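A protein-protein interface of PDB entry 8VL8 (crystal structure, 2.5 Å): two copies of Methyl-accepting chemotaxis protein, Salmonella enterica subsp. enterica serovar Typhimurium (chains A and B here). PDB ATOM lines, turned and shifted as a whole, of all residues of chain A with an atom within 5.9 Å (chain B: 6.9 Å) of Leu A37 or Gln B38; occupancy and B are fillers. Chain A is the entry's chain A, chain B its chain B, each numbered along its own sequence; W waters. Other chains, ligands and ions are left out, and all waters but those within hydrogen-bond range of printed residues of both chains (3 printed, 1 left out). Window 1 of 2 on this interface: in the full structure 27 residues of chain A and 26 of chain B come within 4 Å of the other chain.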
ATOM      1  N   THR A  32     -30.062 -35.203 -21.889  1.00  0.00           N
ATOM      2  CA  THR A  32     -31.399 -34.783 -22.302  1.00  0.00           C
ATOM      3  C   THR A  32     -31.494 -33.256 -22.348  1.00  0.00           C
ATOM      4  O   THR A  32     -31.931 -32.684 -23.348  1.00  0.00           O
ATOM      5  CB  THR A  32     -32.450 -35.381 -21.362  1.00  0.00           C
ATOM      6  OG1 THR A  32     -32.239 -36.800 -21.208  1.00  0.00           O
ATOM      7  CG2 THR A  32     -33.882 -35.118 -21.910  1.00  0.00           C
ATOM      8  N   TRP A  33     -31.100 -32.590 -21.256  1.00  0.00           N
ATOM      9  CA  TRP A  33     -31.098 -31.132 -21.189  1.00  0.00           C
ATOM     10  C   TRP A  33     -30.452 -30.578 -22.445  1.00  0.00           C
ATOM     11  O   TRP A  33     -31.088 -29.866 -23.229  1.00  0.00           O
ATOM     12  CB  TRP A  33     -30.360 -30.710 -19.907  1.00  0.00           C
ATOM     13  CG  TRP A  33     -30.365 -29.227 -19.467  1.00  0.00           C
ATOM     14  CD1 TRP A  33     -29.362 -28.585 -18.822  1.00  0.00           C
ATOM     15  CD2 TRP A  33     -31.404 -28.256 -19.650  1.00  0.00           C
ATOM     16  NE1 TRP A  33     -29.713 -27.284 -18.566  1.00  0.00           N
ATOM     17  CE2 TRP A  33     -30.974 -27.066 -19.056  1.00  0.00           C
ATOM     18  CE3 TRP A  33     -32.682 -28.300 -20.209  1.00  0.00           C
ATOM     19  CZ2 TRP A  33     -31.742 -25.923 -19.051  1.00  0.00           C
ATOM     20  CZ3 TRP A  33     -33.444 -27.162 -20.196  1.00  0.00           C
ATOM     21  CH2 TRP A  33     -32.966 -25.980 -19.647  1.00  0.00           C
ATOM     22  N   VAL A  34     -29.198 -30.974 -22.682  1.00  0.00           N
ATOM     23  CA  VAL A  34     -28.433 -30.417 -23.798  1.00  0.00           C
ATOM     24  C   VAL A  34     -29.162 -30.628 -25.111  1.00  0.00           C
ATOM     25  O   VAL A  34     -29.329 -29.687 -25.886  1.00  0.00           O
ATOM     26  CB  VAL A  34     -27.032 -31.018 -23.850  1.00  0.00           C
ATOM     27  CG1 VAL A  34     -26.431 -30.672 -25.146  1.00  0.00           C
ATOM     28  CG2 VAL A  34     -26.188 -30.468 -22.731  1.00  0.00           C
ATOM     29  N   GLU A  35     -29.637 -31.849 -25.376  1.00  0.00           N
ATOM     30  CA  GLU A  35     -30.307 -32.079 -26.651  1.00  0.00           C
ATOM     31  C   GLU A  35     -31.588 -31.271 -26.779  1.00  0.00           C
ATOM     32  O   GLU A  35     -32.006 -30.910 -27.884  1.00  0.00           O
ATOM     33  CB  GLU A  35     -30.581 -33.564 -26.834  1.00  0.00           C
ATOM     34  CG  GLU A  35     -29.299 -34.375 -27.013  1.00  0.00           C
ATOM     35  CD  GLU A  35     -28.486 -33.888 -28.223  1.00  0.00           C
ATOM     36  OE1 GLU A  35     -29.112 -33.517 -29.249  1.00  0.00           O
ATOM     37  OE2 GLU A  35     -27.245 -33.820 -28.110  1.00  0.00           O
ATOM     38  N   LEU A  36     -32.262 -31.019 -25.668  1.00  0.00           N
ATOM     39  CA  LEU A  36     -33.422 -30.150 -25.734  1.00  0.00           C
ATOM     40  C   LEU A  36     -33.013 -28.750 -26.121  1.00  0.00           C
ATOM     41  O   LEU A  36     -33.714 -28.085 -26.882  1.00  0.00           O
ATOM     42  CB  LEU A  36     -34.135 -30.119 -24.384  1.00  0.00           C
ATOM     43  CG  LEU A  36     -35.185 -31.196 -24.200  1.00  0.00           C
ATOM     44  CD1 LEU A  36     -35.421 -31.397 -22.734  1.00  0.00           C
ATOM     45  CD2 LEU A  36     -36.420 -30.784 -24.913  1.00  0.00           C
ATOM     46  N   LEU A  37     -31.928 -28.273 -25.537  1.00  0.00           N
ATOM     47  CA  LEU A  37     -31.464 -26.923 -25.802  1.00  0.00           C
ATOM     48  C   LEU A  37     -30.904 -26.793 -27.215  1.00  0.00           C
ATOM     49  O   LEU A  37     -31.004 -25.732 -27.819  1.00  0.00           O
ATOM     50  CB  LEU A  37     -30.388 -26.535 -24.784  1.00  0.00           C
ATOM     51  CG  LEU A  37     -30.857 -26.245 -23.348  1.00  0.00           C
ATOM     52  CD1 LEU A  37     -29.605 -26.225 -22.420  1.00  0.00           C
ATOM     53  CD2 LEU A  37     -31.662 -24.951 -23.190  1.00  0.00           C
ATOM     54  N   GLN A  38     -30.321 -27.867 -27.745  1.00  0.00           N
ATOM     55  CA  GLN A  38     -29.892 -27.906 -29.135  1.00  0.00           C
ATOM     56  C   GLN A  38     -31.087 -27.996 -30.068  1.00  0.00           C
ATOM     57  O   GLN A  38     -31.160 -27.281 -31.066  1.00  0.00           O
ATOM     58  CB  GLN A  38     -28.932 -29.100 -29.340  1.00  0.00           C
ATOM     59  CG  GLN A  38     -27.519 -28.697 -28.956  1.00  0.00           C
ATOM     60  CD  GLN A  38     -26.518 -29.811 -28.891  1.00  0.00           C
ATOM     61  OE1 GLN A  38     -25.335 -29.588 -29.149  1.00  0.00           O
ATOM     62  NE2 GLN A  38     -26.958 -31.003 -28.516  1.00  0.00           N
ATOM     63  N   THR A  39     -32.034 -28.873 -29.780  1.00  0.00           N
ATOM     64  CA  THR A  39     -33.249 -28.826 -30.579  1.00  0.00           C
ATOM     65  C   THR A  39     -33.818 -27.399 -30.585  1.00  0.00           C
ATOM     66  O   THR A  39     -34.165 -26.855 -31.639  1.00  0.00           O
ATOM     67  CB  THR A  39     -34.303 -29.786 -30.064  1.00  0.00           C
ATOM     68  OG1 THR A  39     -33.813 -31.127 -29.984  1.00  0.00           O
ATOM     69  CG2 THR A  39     -35.463 -29.768 -31.005  1.00  0.00           C
ATOM     70  N   ARG A  40     -33.961 -26.778 -29.410  1.00  0.00           N
ATOM     71  CA  ARG A  40     -34.621 -25.463 -29.404  1.00  0.00           C
ATOM     72  C   ARG A  40     -33.880 -24.467 -30.301  1.00  0.00           C
ATOM     73  O   ARG A  40     -34.488 -23.736 -31.087  1.00  0.00           O
ATOM     74  CB  ARG A  40     -34.737 -24.909 -27.988  1.00  0.00           C
ATOM     75  CG  ARG A  40     -35.724 -23.750 -27.932  1.00  0.00           C
ATOM     76  CD  ARG A  40     -35.887 -23.249 -26.493  1.00  0.00           C
ATOM     77  NE  ARG A  40     -36.651 -22.014 -26.463  1.00  0.00           N
ATOM     78  CZ  ARG A  40     -36.615 -21.170 -25.457  1.00  0.00           C
ATOM     79  NH1 ARG A  40     -35.884 -21.422 -24.381  1.00  0.00           N
ATOM     80  NH2 ARG A  40     -37.336 -20.059 -25.526  1.00  0.00           N
ATOM     81  N   ASN A  41     -32.561 -24.471 -30.254  1.00  0.00           N
ATOM     82  CA  ASN A  41     -31.826 -23.441 -31.002  1.00  0.00           C
ATOM     83  C   ASN A  41     -31.917 -23.674 -32.503  1.00  0.00           C
ATOM     84  O   ASN A  41     -32.255 -22.769 -33.273  1.00  0.00           O
ATOM     85  CB  ASN A  41     -30.378 -23.408 -30.525  1.00  0.00           C
ATOM     86  CG  ASN A  41     -29.502 -22.617 -31.448  1.00  0.00           C
ATOM     87  OD1 ASN A  41     -28.735 -23.173 -32.248  1.00  0.00           O
ATOM     88  ND2 ASN A  41     -29.647 -21.322 -31.385  1.00  0.00           N
ATOM     89  N   THR A  42     -31.687 -24.900 -32.927  1.00  0.00           N
ATOM     90  CA  THR A  42     -31.840 -25.257 -34.325  1.00  0.00           C
ATOM     91  C   THR A  42     -33.198 -24.853 -34.863  1.00  0.00           C
ATOM     92  O   THR A  42     -33.304 -24.257 -35.944  1.00  0.00           O
ATOM     93  CB  THR A  42     -31.595 -26.762 -34.455  1.00  0.00           C
ATOM     94  OG1 THR A  42     -30.286 -27.018 -33.934  1.00  0.00           O
ATOM     95  CG2 THR A  42     -31.691 -27.161 -35.870  1.00  0.00           C
ATOM     96  N   TYR A 108     -42.015 -29.844 -21.900  1.00  0.00           N
ATOM     97  CA  TYR A 108     -41.002 -29.174 -22.731  1.00  0.00           C
ATOM     98  C   TYR A 108     -40.832 -29.889 -24.070  1.00  0.00           C
ATOM     99  O   TYR A 108     -41.121 -29.336 -25.130  1.00  0.00           O
ATOM    100  CB  TYR A 108     -39.686 -29.096 -21.962  1.00  0.00           C
ATOM    101  CG  TYR A 108     -38.613 -28.213 -22.571  1.00  0.00           C
ATOM    102  CD1 TYR A 108     -38.871 -27.374 -23.650  1.00  0.00           C
ATOM    103  CD2 TYR A 108     -37.332 -28.254 -22.088  1.00  0.00           C
ATOM    104  CE1 TYR A 108     -37.825 -26.578 -24.228  1.00  0.00           C
ATOM    105  CE2 TYR A 108     -36.328 -27.466 -22.609  1.00  0.00           C
ATOM    106  CZ  TYR A 108     -36.555 -26.637 -23.675  1.00  0.00           C
ATOM    107  OH  TYR A 108     -35.473 -25.896 -24.190  1.00  0.00           O
ATOM    108  N   LEU A 112     -41.549 -28.669 -27.976  1.00  0.00           N
ATOM    109  CA  LEU A 112     -40.639 -28.589 -29.119  1.00  0.00           C
ATOM    110  C   LEU A 112     -41.154 -29.445 -30.252  1.00  0.00           C
ATOM    111  O   LEU A 112     -40.995 -29.101 -31.430  1.00  0.00           O
ATOM    112  CB  LEU A 112     -39.226 -29.040 -28.771  1.00  0.00           C
ATOM    113  CG  LEU A 112     -38.569 -28.238 -27.693  1.00  0.00           C
ATOM    114  CD1 LEU A 112     -37.213 -28.667 -27.557  1.00  0.00           C
ATOM    115  CD2 LEU A 112     -38.563 -26.755 -27.867  1.00  0.00           C
ATOM    116  N   GLN A 133     -40.215 -20.666 -23.487  1.00  0.00           N
ATOM    117  CA  GLN A 133     -39.316 -20.285 -22.400  1.00  0.00           C
ATOM    118  C   GLN A 133     -39.890 -20.700 -21.024  1.00  0.00           C
ATOM    119  O   GLN A 133     -39.147 -21.162 -20.147  1.00  0.00           O
ATOM    120  CB  GLN A 133     -39.048 -18.792 -22.441  1.00  0.00           C
ATOM    121  CG  GLN A 133     -37.930 -18.378 -21.496  1.00  0.00           C
ATOM    122  CD  GLN A 133     -36.557 -18.780 -21.997  1.00  0.00           C
ATOM    123  OE1 GLN A 133     -36.243 -18.682 -23.183  1.00  0.00           O
ATOM    124  NE2 GLN A 133     -35.715 -19.150 -21.082  1.00  0.00           N
ATOM    125  N   GLN A 136     -39.395 -24.437 -20.623  1.00  0.00           N
ATOM    126  CA  GLN A 136     -38.021 -24.785 -20.370  1.00  0.00           C
ATOM    127  C   GLN A 136     -37.624 -24.422 -18.956  1.00  0.00           C
ATOM    128  O   GLN A 136     -36.871 -25.161 -18.307  1.00  0.00           O
ATOM    129  CB  GLN A 136     -37.116 -24.048 -21.368  1.00  0.00           C
ATOM    130  CG  GLN A 136     -35.677 -24.361 -21.220  1.00  0.00           C
ATOM    131  CD  GLN A 136     -34.778 -23.500 -22.219  1.00  0.00           C
ATOM    132  OE1 GLN A 136     -34.843 -23.609 -23.455  1.00  0.00           O
ATOM    133  NE2 GLN A 136     -33.938 -22.710 -21.652  1.00  0.00           N
ATOM    134  N   ASP A 137     -38.038 -23.225 -18.502  1.00  0.00           N
ATOM    135  CA  ASP A 137     -37.681 -22.761 -17.171  1.00  0.00           C
ATOM    136  C   ASP A 137     -38.266 -23.691 -16.106  1.00  0.00           C
ATOM    137  O   ASP A 137     -37.631 -23.931 -15.078  1.00  0.00           O
ATOM    138  CB  ASP A 137     -38.219 -21.346 -16.888  1.00  0.00           C
ATOM    139  CG  ASP A 137     -37.684 -20.271 -17.813  1.00  0.00           C
ATOM    140  OD1 ASP A 137     -36.769 -20.584 -18.564  1.00  0.00           O
ATOM    141  OD2 ASP A 137     -38.249 -19.124 -17.794  1.00  0.00           O
ATOM    142  N   GLU A 140     -35.880 -26.519 -16.182  1.00  0.00           N
ATOM    143  CA  GLU A 140     -34.584 -26.199 -15.615  1.00  0.00           C
ATOM    144  C   GLU A 140     -34.662 -26.063 -14.084  1.00  0.00           C
ATOM    145  O   GLU A 140     -33.765 -26.518 -13.361  1.00  0.00           O
ATOM    146  CB  GLU A 140     -34.066 -24.937 -16.297  1.00  0.00           C
ATOM    147  CG  GLU A 140     -32.673 -24.557 -15.913  1.00  0.00           C
ATOM    148  CD  GLU A 140     -32.162 -23.229 -16.516  1.00  0.00           C
ATOM    149  OE1 GLU A 140     -32.941 -22.435 -17.105  1.00  0.00           O
ATOM    150  OE2 GLU A 140     -30.950 -22.980 -16.350  1.00  0.00           O
ATOM    151  N   ALA B  31     -21.986 -26.017 -16.664  1.00  0.00           N
ATOM    152  CA  ALA B  31     -22.821 -24.833 -16.540  1.00  0.00           C
ATOM    153  C   ALA B  31     -22.503 -23.823 -17.634  1.00  0.00           C
ATOM    154  O   ALA B  31     -23.411 -23.139 -18.115  1.00  0.00           O
ATOM    155  CB  ALA B  31     -22.658 -24.203 -15.161  1.00  0.00           C
ATOM    156  N   THR B  32     -21.231 -23.721 -18.049  1.00  0.00           N
ATOM    157  CA  THR B  32     -20.861 -22.859 -19.185  1.00  0.00           C
ATOM    158  C   THR B  32     -21.484 -23.349 -20.492  1.00  0.00           C
ATOM    159  O   THR B  32     -22.196 -22.605 -21.160  1.00  0.00           O
ATOM    160  CB  THR B  32     -19.343 -22.789 -19.298  1.00  0.00           C
ATOM    161  OG1 THR B  32     -18.761 -22.742 -17.978  1.00  0.00           O
ATOM    162  CG2 THR B  32     -18.878 -21.539 -20.087  1.00  0.00           C
ATOM    163  N   TRP B  33     -21.228 -24.597 -20.875  1.00  0.00           N
ATOM    164  CA  TRP B  33     -21.914 -25.224 -22.001  1.00  0.00           C
ATOM    165  C   TRP B  33     -23.383 -24.821 -22.042  1.00  0.00           C
ATOM    166  O   TRP B  33     -23.825 -24.136 -22.964  1.00  0.00           O
ATOM    167  CB  TRP B  33     -21.773 -26.769 -21.897  1.00  0.00           C
ATOM    168  CG  TRP B  33     -22.309 -27.654 -23.068  1.00  0.00           C
ATOM    169  CD1 TRP B  33     -22.883 -28.904 -22.945  1.00  0.00           C
ATOM    170  CD2 TRP B  33     -22.303 -27.371 -24.495  1.00  0.00           C
ATOM    171  NE1 TRP B  33     -23.233 -29.397 -24.179  1.00  0.00           N
ATOM    172  CE2 TRP B  33     -22.884 -28.487 -25.146  1.00  0.00           C
ATOM    173  CE3 TRP B  33     -21.858 -26.294 -25.274  1.00  0.00           C
ATOM    174  CZ2 TRP B  33     -23.023 -28.565 -26.534  1.00  0.00           C
ATOM    175  CZ3 TRP B  33     -22.017 -26.366 -26.659  1.00  0.00           C
ATOM    176  CH2 TRP B  33     -22.592 -27.493 -27.272  1.00  0.00           C
ATOM    177  N   VAL B  34     -24.135 -25.231 -21.007  1.00  0.00           N
ATOM    178  CA  VAL B  34     -25.578 -25.002 -20.944  1.00  0.00           C
ATOM    179  C   VAL B  34     -25.915 -23.567 -21.279  1.00  0.00           C
ATOM    180  O   VAL B  34     -26.941 -23.279 -21.902  1.00  0.00           O
ATOM    181  CB  VAL B  34     -26.120 -25.337 -19.537  1.00  0.00           C
ATOM    182  CG1 VAL B  34     -27.601 -25.119 -19.499  1.00  0.00           C
ATOM    183  CG2 VAL B  34     -25.791 -26.728 -19.174  1.00  0.00           C
ATOM    184  N   GLU B  35     -25.105 -22.646 -20.783  1.00  0.00           N
ATOM    185  CA  GLU B  35     -25.382 -21.241 -20.941  1.00  0.00           C
ATOM    186  C   GLU B  35     -24.972 -20.716 -22.315  1.00  0.00           C
ATOM    187  O   GLU B  35     -25.608 -19.781 -22.856  1.00  0.00           O
ATOM    188  CB  GLU B  35     -24.656 -20.510 -19.843  1.00  0.00           C
ATOM    189  CG  GLU B  35     -25.406 -19.345 -19.274  1.00  0.00           C
ATOM    190  CD  GLU B  35     -26.683 -19.740 -18.567  1.00  0.00           C
ATOM    191  OE1 GLU B  35     -26.583 -20.607 -17.683  1.00  0.00           O
ATOM    192  OE2 GLU B  35     -27.761 -19.157 -18.874  1.00  0.00           O
ATOM    193  N   LEU B  36     -23.885 -21.262 -22.871  1.00  0.00           N
ATOM    194  CA  LEU B  36     -23.564 -20.959 -24.263  1.00  0.00           C
ATOM    195  C   LEU B  36     -24.743 -21.318 -25.158  1.00  0.00           C
ATOM    196  O   LEU B  36     -25.073 -20.574 -26.075  1.00  0.00           O
ATOM    197  CB  LEU B  36     -22.301 -21.712 -24.699  1.00  0.00           C
ATOM    198  CG  LEU B  36     -20.974 -21.128 -24.218  1.00  0.00           C
ATOM    199  CD1 LEU B  36     -19.814 -22.131 -24.287  1.00  0.00           C
ATOM    200  CD2 LEU B  36     -20.618 -19.873 -24.992  1.00  0.00           C
ATOM    201  N   LEU B  37     -25.440 -22.419 -24.844  1.00  0.00           N
ATOM    202  CA  LEU B  37     -26.565 -22.871 -25.670  1.00  0.00           C
ATOM    203  C   LEU B  37     -27.806 -22.007 -25.478  1.00  0.00           C
ATOM    204  O   LEU B  37     -28.535 -21.735 -26.441  1.00  0.00           O
ATOM    205  CB  LEU B  37     -26.899 -24.335 -25.332  1.00  0.00           C
ATOM    206  CG  LEU B  37     -25.963 -25.474 -25.753  1.00  0.00           C
ATOM    207  CD1 LEU B  37     -26.307 -26.786 -25.022  1.00  0.00           C
ATOM    208  CD2 LEU B  37     -25.972 -25.763 -27.246  1.00  0.00           C
ATOM    209  N   GLN B  38     -28.126 -21.612 -24.240  1.00  0.00           N
ATOM    210  CA  GLN B  38     -29.293 -20.733 -24.064  1.00  0.00           C
ATOM    211  C   GLN B  38     -29.072 -19.392 -24.737  1.00  0.00           C
ATOM    212  O   GLN B  38     -30.014 -18.813 -25.286  1.00  0.00           O
ATOM    213  CB  GLN B  38     -29.651 -20.531 -22.575  1.00  0.00           C
ATOM    214  CG  GLN B  38     -30.194 -21.831 -21.966  1.00  0.00           C
ATOM    215  CD  GLN B  38     -30.463 -21.791 -20.481  1.00  0.00           C
ATOM    216  OE1 GLN B  38     -31.616 -21.908 -20.049  1.00  0.00           O
ATOM    217  NE2 GLN B  38     -29.406 -21.700 -19.687  1.00  0.00           N
ATOM    218  N   THR B  39     -27.835 -18.897 -24.740  1.00  0.00           N
ATOM    219  CA  THR B  39     -27.557 -17.620 -25.406  1.00  0.00           C
ATOM    220  C   THR B  39     -27.770 -17.719 -26.925  1.00  0.00           C
ATOM    221  O   THR B  39     -28.342 -16.831 -27.552  1.00  0.00           O
ATOM    222  CB  THR B  39     -26.125 -17.195 -25.093  1.00  0.00           C
ATOM    223  OG1 THR B  39     -25.919 -17.236 -23.688  1.00  0.00           O
ATOM    224  CG2 THR B  39     -25.809 -15.808 -25.705  1.00  0.00           C
ATOM    225  N   ARG B  40     -27.277 -18.783 -27.539  1.00  0.00           N
ATOM    226  CA  ARG B  40     -27.449 -18.935 -28.973  1.00  0.00           C
ATOM    227  C   ARG B  40     -28.926 -18.949 -29.338  1.00  0.00           C
ATOM    228  O   ARG B  40     -29.360 -18.268 -30.275  1.00  0.00           O
ATOM    229  CB  ARG B  40     -26.731 -20.224 -29.371  1.00  0.00           C
ATOM    230  CG  ARG B  40     -26.328 -20.255 -30.799  1.00  0.00           C
ATOM    231  CD  ARG B  40     -25.937 -21.668 -31.282  1.00  0.00           C
ATOM    232  NE  ARG B  40     -25.962 -21.716 -32.736  1.00  0.00           N
ATOM    233  CZ  ARG B  40     -25.706 -22.789 -33.462  1.00  0.00           C
ATOM    234  NH1 ARG B  40     -25.339 -23.927 -32.899  1.00  0.00           N
ATOM    235  NH2 ARG B  40     -25.799 -22.708 -34.791  1.00  0.00           N
ATOM    236  N   ASN B  41     -29.722 -19.647 -28.541  1.00  0.00           N
ATOM    237  CA  ASN B  41     -31.139 -19.784 -28.828  1.00  0.00           C
ATOM    238  C   ASN B  41     -31.797 -18.429 -28.690  1.00  0.00           C
ATOM    239  O   ASN B  41     -32.469 -17.935 -29.612  1.00  0.00           O
ATOM    240  CB  ASN B  41     -31.754 -20.842 -27.893  1.00  0.00           C
ATOM    241  CG  ASN B  41     -33.243 -20.958 -28.074  1.00  0.00           C
ATOM    242  OD1 ASN B  41     -33.738 -21.606 -29.013  1.00  0.00           O
ATOM    243  ND2 ASN B  41     -33.973 -20.309 -27.203  1.00  0.00           N
ATOM    244  N   THR B  42     -31.467 -17.734 -27.607  1.00  0.00           N
ATOM    245  CA  THR B  42     -32.003 -16.388 -27.435  1.00  0.00           C
ATOM    246  C   THR B  42     -31.626 -15.509 -28.616  1.00  0.00           C
ATOM    247  O   THR B  42     -32.500 -14.890 -29.224  1.00  0.00           O
ATOM    248  CB  THR B  42     -31.551 -15.790 -26.108  1.00  0.00           C
ATOM    249  OG1 THR B  42     -31.913 -16.664 -25.018  1.00  0.00           O
ATOM    250  CG2 THR B  42     -32.282 -14.494 -25.932  1.00  0.00           C
ATOM    251  N   LEU B  43     -30.342 -15.501 -29.020  1.00  0.00           N
ATOM    252  CA  LEU B  43     -29.950 -14.688 -30.191  1.00  0.00           C
ATOM    253  C   LEU B  43     -30.797 -15.019 -31.417  1.00  0.00           C
ATOM    254  O   LEU B  43     -31.311 -14.117 -32.090  1.00  0.00           O
ATOM    255  CB  LEU B  43     -28.476 -14.874 -30.528  1.00  0.00           C
ATOM    256  CG  LEU B  43     -27.557 -14.261 -29.474  1.00  0.00           C
ATOM    257  CD1 LEU B  43     -26.162 -14.716 -29.619  1.00  0.00           C
ATOM    258  CD2 LEU B  43     -27.650 -12.751 -29.574  1.00  0.00           C
ATOM    259  N   ALA B  70     -29.863 -12.082 -23.907  1.00  0.00           N
ATOM    260  CA  ALA B  70     -28.638 -12.612 -24.501  1.00  0.00           C
ATOM    261  C   ALA B  70     -27.404 -11.937 -23.932  1.00  0.00           C
ATOM    262  O   ALA B  70     -26.413 -12.607 -23.602  1.00  0.00           O
ATOM    263  CB  ALA B  70     -28.694 -12.437 -26.019  1.00  0.00           C
ATOM    264  N   THR B  73     -27.005 -13.416 -20.521  1.00  0.00           N
ATOM    265  CA  THR B  73     -26.520 -14.806 -20.361  1.00  0.00           C
ATOM    266  C   THR B  73     -25.090 -15.003 -20.880  1.00  0.00           C
ATOM    267  O   THR B  73     -24.401 -15.957 -20.465  1.00  0.00           O
ATOM    268  CB  THR B  73     -27.427 -15.828 -21.046  1.00  0.00           C
ATOM    269  OG1 THR B  73     -27.700 -15.437 -22.397  1.00  0.00           O
ATOM    270  CG2 THR B  73     -28.740 -16.023 -20.286  1.00  0.00           C
ATOM    271  N   LEU B  76     -23.105 -14.322 -17.812  1.00  0.00           N
ATOM    272  CA  LEU B  76     -23.152 -15.510 -16.965  1.00  0.00           C
ATOM    273  C   LEU B  76     -22.205 -16.582 -17.488  1.00  0.00           C
ATOM    274  O   LEU B  76     -21.634 -17.363 -16.701  1.00  0.00           O
ATOM    275  CB  LEU B  76     -24.563 -16.114 -16.900  1.00  0.00           C
ATOM    276  CG  LEU B  76     -25.723 -15.365 -16.257  1.00  0.00           C
ATOM    277  CD1 LEU B  76     -27.039 -16.090 -16.582  1.00  0.00           C
ATOM    278  CD2 LEU B  76     -25.468 -15.256 -14.743  1.00  0.00           C
ATOM    279  N   TYR B 108     -16.087 -19.694 -29.550  1.00  0.00           N
ATOM    280  CA  TYR B 108     -17.542 -19.790 -29.472  1.00  0.00           C
ATOM    281  C   TYR B 108     -18.115 -18.584 -28.748  1.00  0.00           C
ATOM    282  O   TYR B 108     -18.969 -17.861 -29.288  1.00  0.00           O
ATOM    283  CB  TYR B 108     -17.906 -21.105 -28.779  1.00  0.00           C
ATOM    284  CG  TYR B 108     -19.378 -21.470 -28.806  1.00  0.00           C
ATOM    285  CD1 TYR B 108     -20.253 -20.828 -29.640  1.00  0.00           C
ATOM    286  CD2 TYR B 108     -19.879 -22.418 -27.955  1.00  0.00           C
ATOM    287  CE1 TYR B 108     -21.597 -21.142 -29.662  1.00  0.00           C
ATOM    288  CE2 TYR B 108     -21.236 -22.761 -27.984  1.00  0.00           C
ATOM    289  CZ  TYR B 108     -22.083 -22.103 -28.830  1.00  0.00           C
ATOM    290  OH  TYR B 108     -23.430 -22.451 -28.861  1.00  0.00           O
ATOM    291  N   GLN B 136     -19.572 -24.132 -32.154  1.00  0.00           N
ATOM    292  CA  GLN B 136     -20.219 -24.955 -31.135  1.00  0.00           C
ATOM    293  C   GLN B 136     -19.750 -26.403 -31.233  1.00  0.00           C
ATOM    294  O   GLN B 136     -19.321 -27.012 -30.238  1.00  0.00           O
ATOM    295  CB  GLN B 136     -21.737 -24.863 -31.292  1.00  0.00           C
ATOM    296  CG  GLN B 136     -22.427 -25.540 -30.114  1.00  0.00           C
ATOM    297  CD  GLN B 136     -23.914 -25.584 -30.302  1.00  0.00           C
ATOM    298  OE1 GLN B 136     -24.618 -24.595 -30.097  1.00  0.00           O
ATOM    299  NE2 GLN B 136     -24.399 -26.719 -30.772  1.00  0.00           N
HETATM  300  O   HOH W   1     -34.724 -16.892 -24.486  1.00  0.00           O
HETATM  301  O   HOH W   2     -23.194 -28.775 -31.263  1.00  0.00           O
HETATM  302  O   HOH W   3     -32.644 -20.193 -21.790  1.00  0.00           O
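Val A34 touches Leu B37, and with the chains exchanged Leu A37 touches Val B34. Gln A38 touches Gln B136, and with the chains exchanged Gln A136 touches Gln B38. Arg A40 touches Asn B41, and with the chains exchanged Asn A41 touches Arg B40. Asn A41 touches its own counterpart, Asn B41. Positions printed for both chains: 32, 33, 34, 35, 36, 37, 38, 39, 40, 41, 42, 108 and 136.
Printed residues of chain B that touch a printed residue of chain A: Trp B33, Val B34, Leu B37, Gln B38, Arg B40, Asn B41 and Gln B136. Hydrophobic or aromatic side chains of chain A that line the printed part of chain B: Trp A33, Val A34 and Leu A37. Along chain A the printed residues that touch a printed residue of chain B span positions 33 to 140. Among the printed residues, no Asp or Glu carboxylate lies within 4 Å of a Lys or Arg side-chain nitrogen of the other chain.
Trp A33 touches Val B34 (NE1 to CG1, 3.2 Å). Val A34 touches Trp B33. Val A34 touches Leu B37. CG1 of Val B34 touches CD1 of Leu A37 (3.7 Å). Leu A37 touches Gln B38 (CD2 to CG, 3.7 Å). Trp B33 touches Gln A38 (CZ2 to OE1, 3.6 Å). Gln A38 touches Leu B37.
The side-chain hydroxyl (OG1) of Thr A42 lies within hydrogen-bond range of the backbone carbonyl oxygen (O) of Gln A38, 3.0 Å away. The guanidinium group (NH1) of Arg A40 sits at hydrogen-bond distance from the side-chain amide oxygen (OE1) of Gln A136 (2.6 Å). OH of Tyr A108 lies within hydrogen-bond range of OE1 of Gln A136, 2.5 Å away. The side-chain amide nitrogen (NE2) of Gln B38 is in hydrogen-bond range of the side-chain carboxylate (OE2) of Glu B35 (3.1 Å). The side-chain hydroxyl (OG1) of Thr B42 sits at hydrogen-bond distance from the backbone carbonyl oxygen (O) of Gln B38, at 2.9 Å. The side-chain hydroxyl of Tyr B108 lies within hydrogen-bond range of the side-chain amide oxygen of Gln B136 (2.7 Å).
NE2 of Gln B136 is in hydrogen-bond range of OE1 of Gln A38 (3.4 Å). The backbone carbonyl oxygen of Arg A40 sits close to the side-chain amide oxygen of Asn B41. NE of Arg B40 sits at hydrogen-bond distance from OD1 of Asn A41, at 3.2 Å. The side-chain amide nitrogen (ND2) of Asn A41 lies close to the backbone NH (N) of Asn B41. NE2 of Gln A136 sits at hydrogen-bond distance from OE1 of Gln B38 (2.9 Å). The side-chain amide oxygen (OE1) of Gln B38 lies close to the side-chain carboxylate (OE1) of Glu A140.
Leu A37 touches just these residues of chain B: Val B34 and Gln B38. Of the printed residues of chain A, Gln B38 touches Leu A37 (3.7 Å), Gln A136 (2.9 Å) and Glu A140 (3.3 Å). Of the printed residues of chain A, Asn B41 touches Arg A40 and Asn A41. Of the printed residues of chain B, Asn A41 touches Arg B40 and Asn B41. Of the printed residues of chain B, Val A34 touches Trp B33 (3.5 Å) and Leu B37 (3.9 Å). Leu B36 touches none of the printed residues of chain A. The nearest residue of chain A that does not touch Gln B38 is Trp A33 (4.1 Å). The nearest printed residue of chain A that does not touch Gln B136 is Asn A41 (4.9 Å).
Water W2 bridges the side-chain amide nitrogen (NE2) of Gln B136 and the side-chain amide oxygen (OE1) of Gln A38. Water W3 lies within hydrogen-bond range of the side-chain amide oxygen (OE1) of Gln B38 (2.7 Å), the side-chain amide nitrogen (NE2) of Gln A136 (2.8 Å) and the side-chain amide nitrogen (NE2) of Gln A133 (3.3 Å). Water W1 bridges OE1 of Gln A133 (2.7 Å) and OG1 of Thr B42 (2.9 Å).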
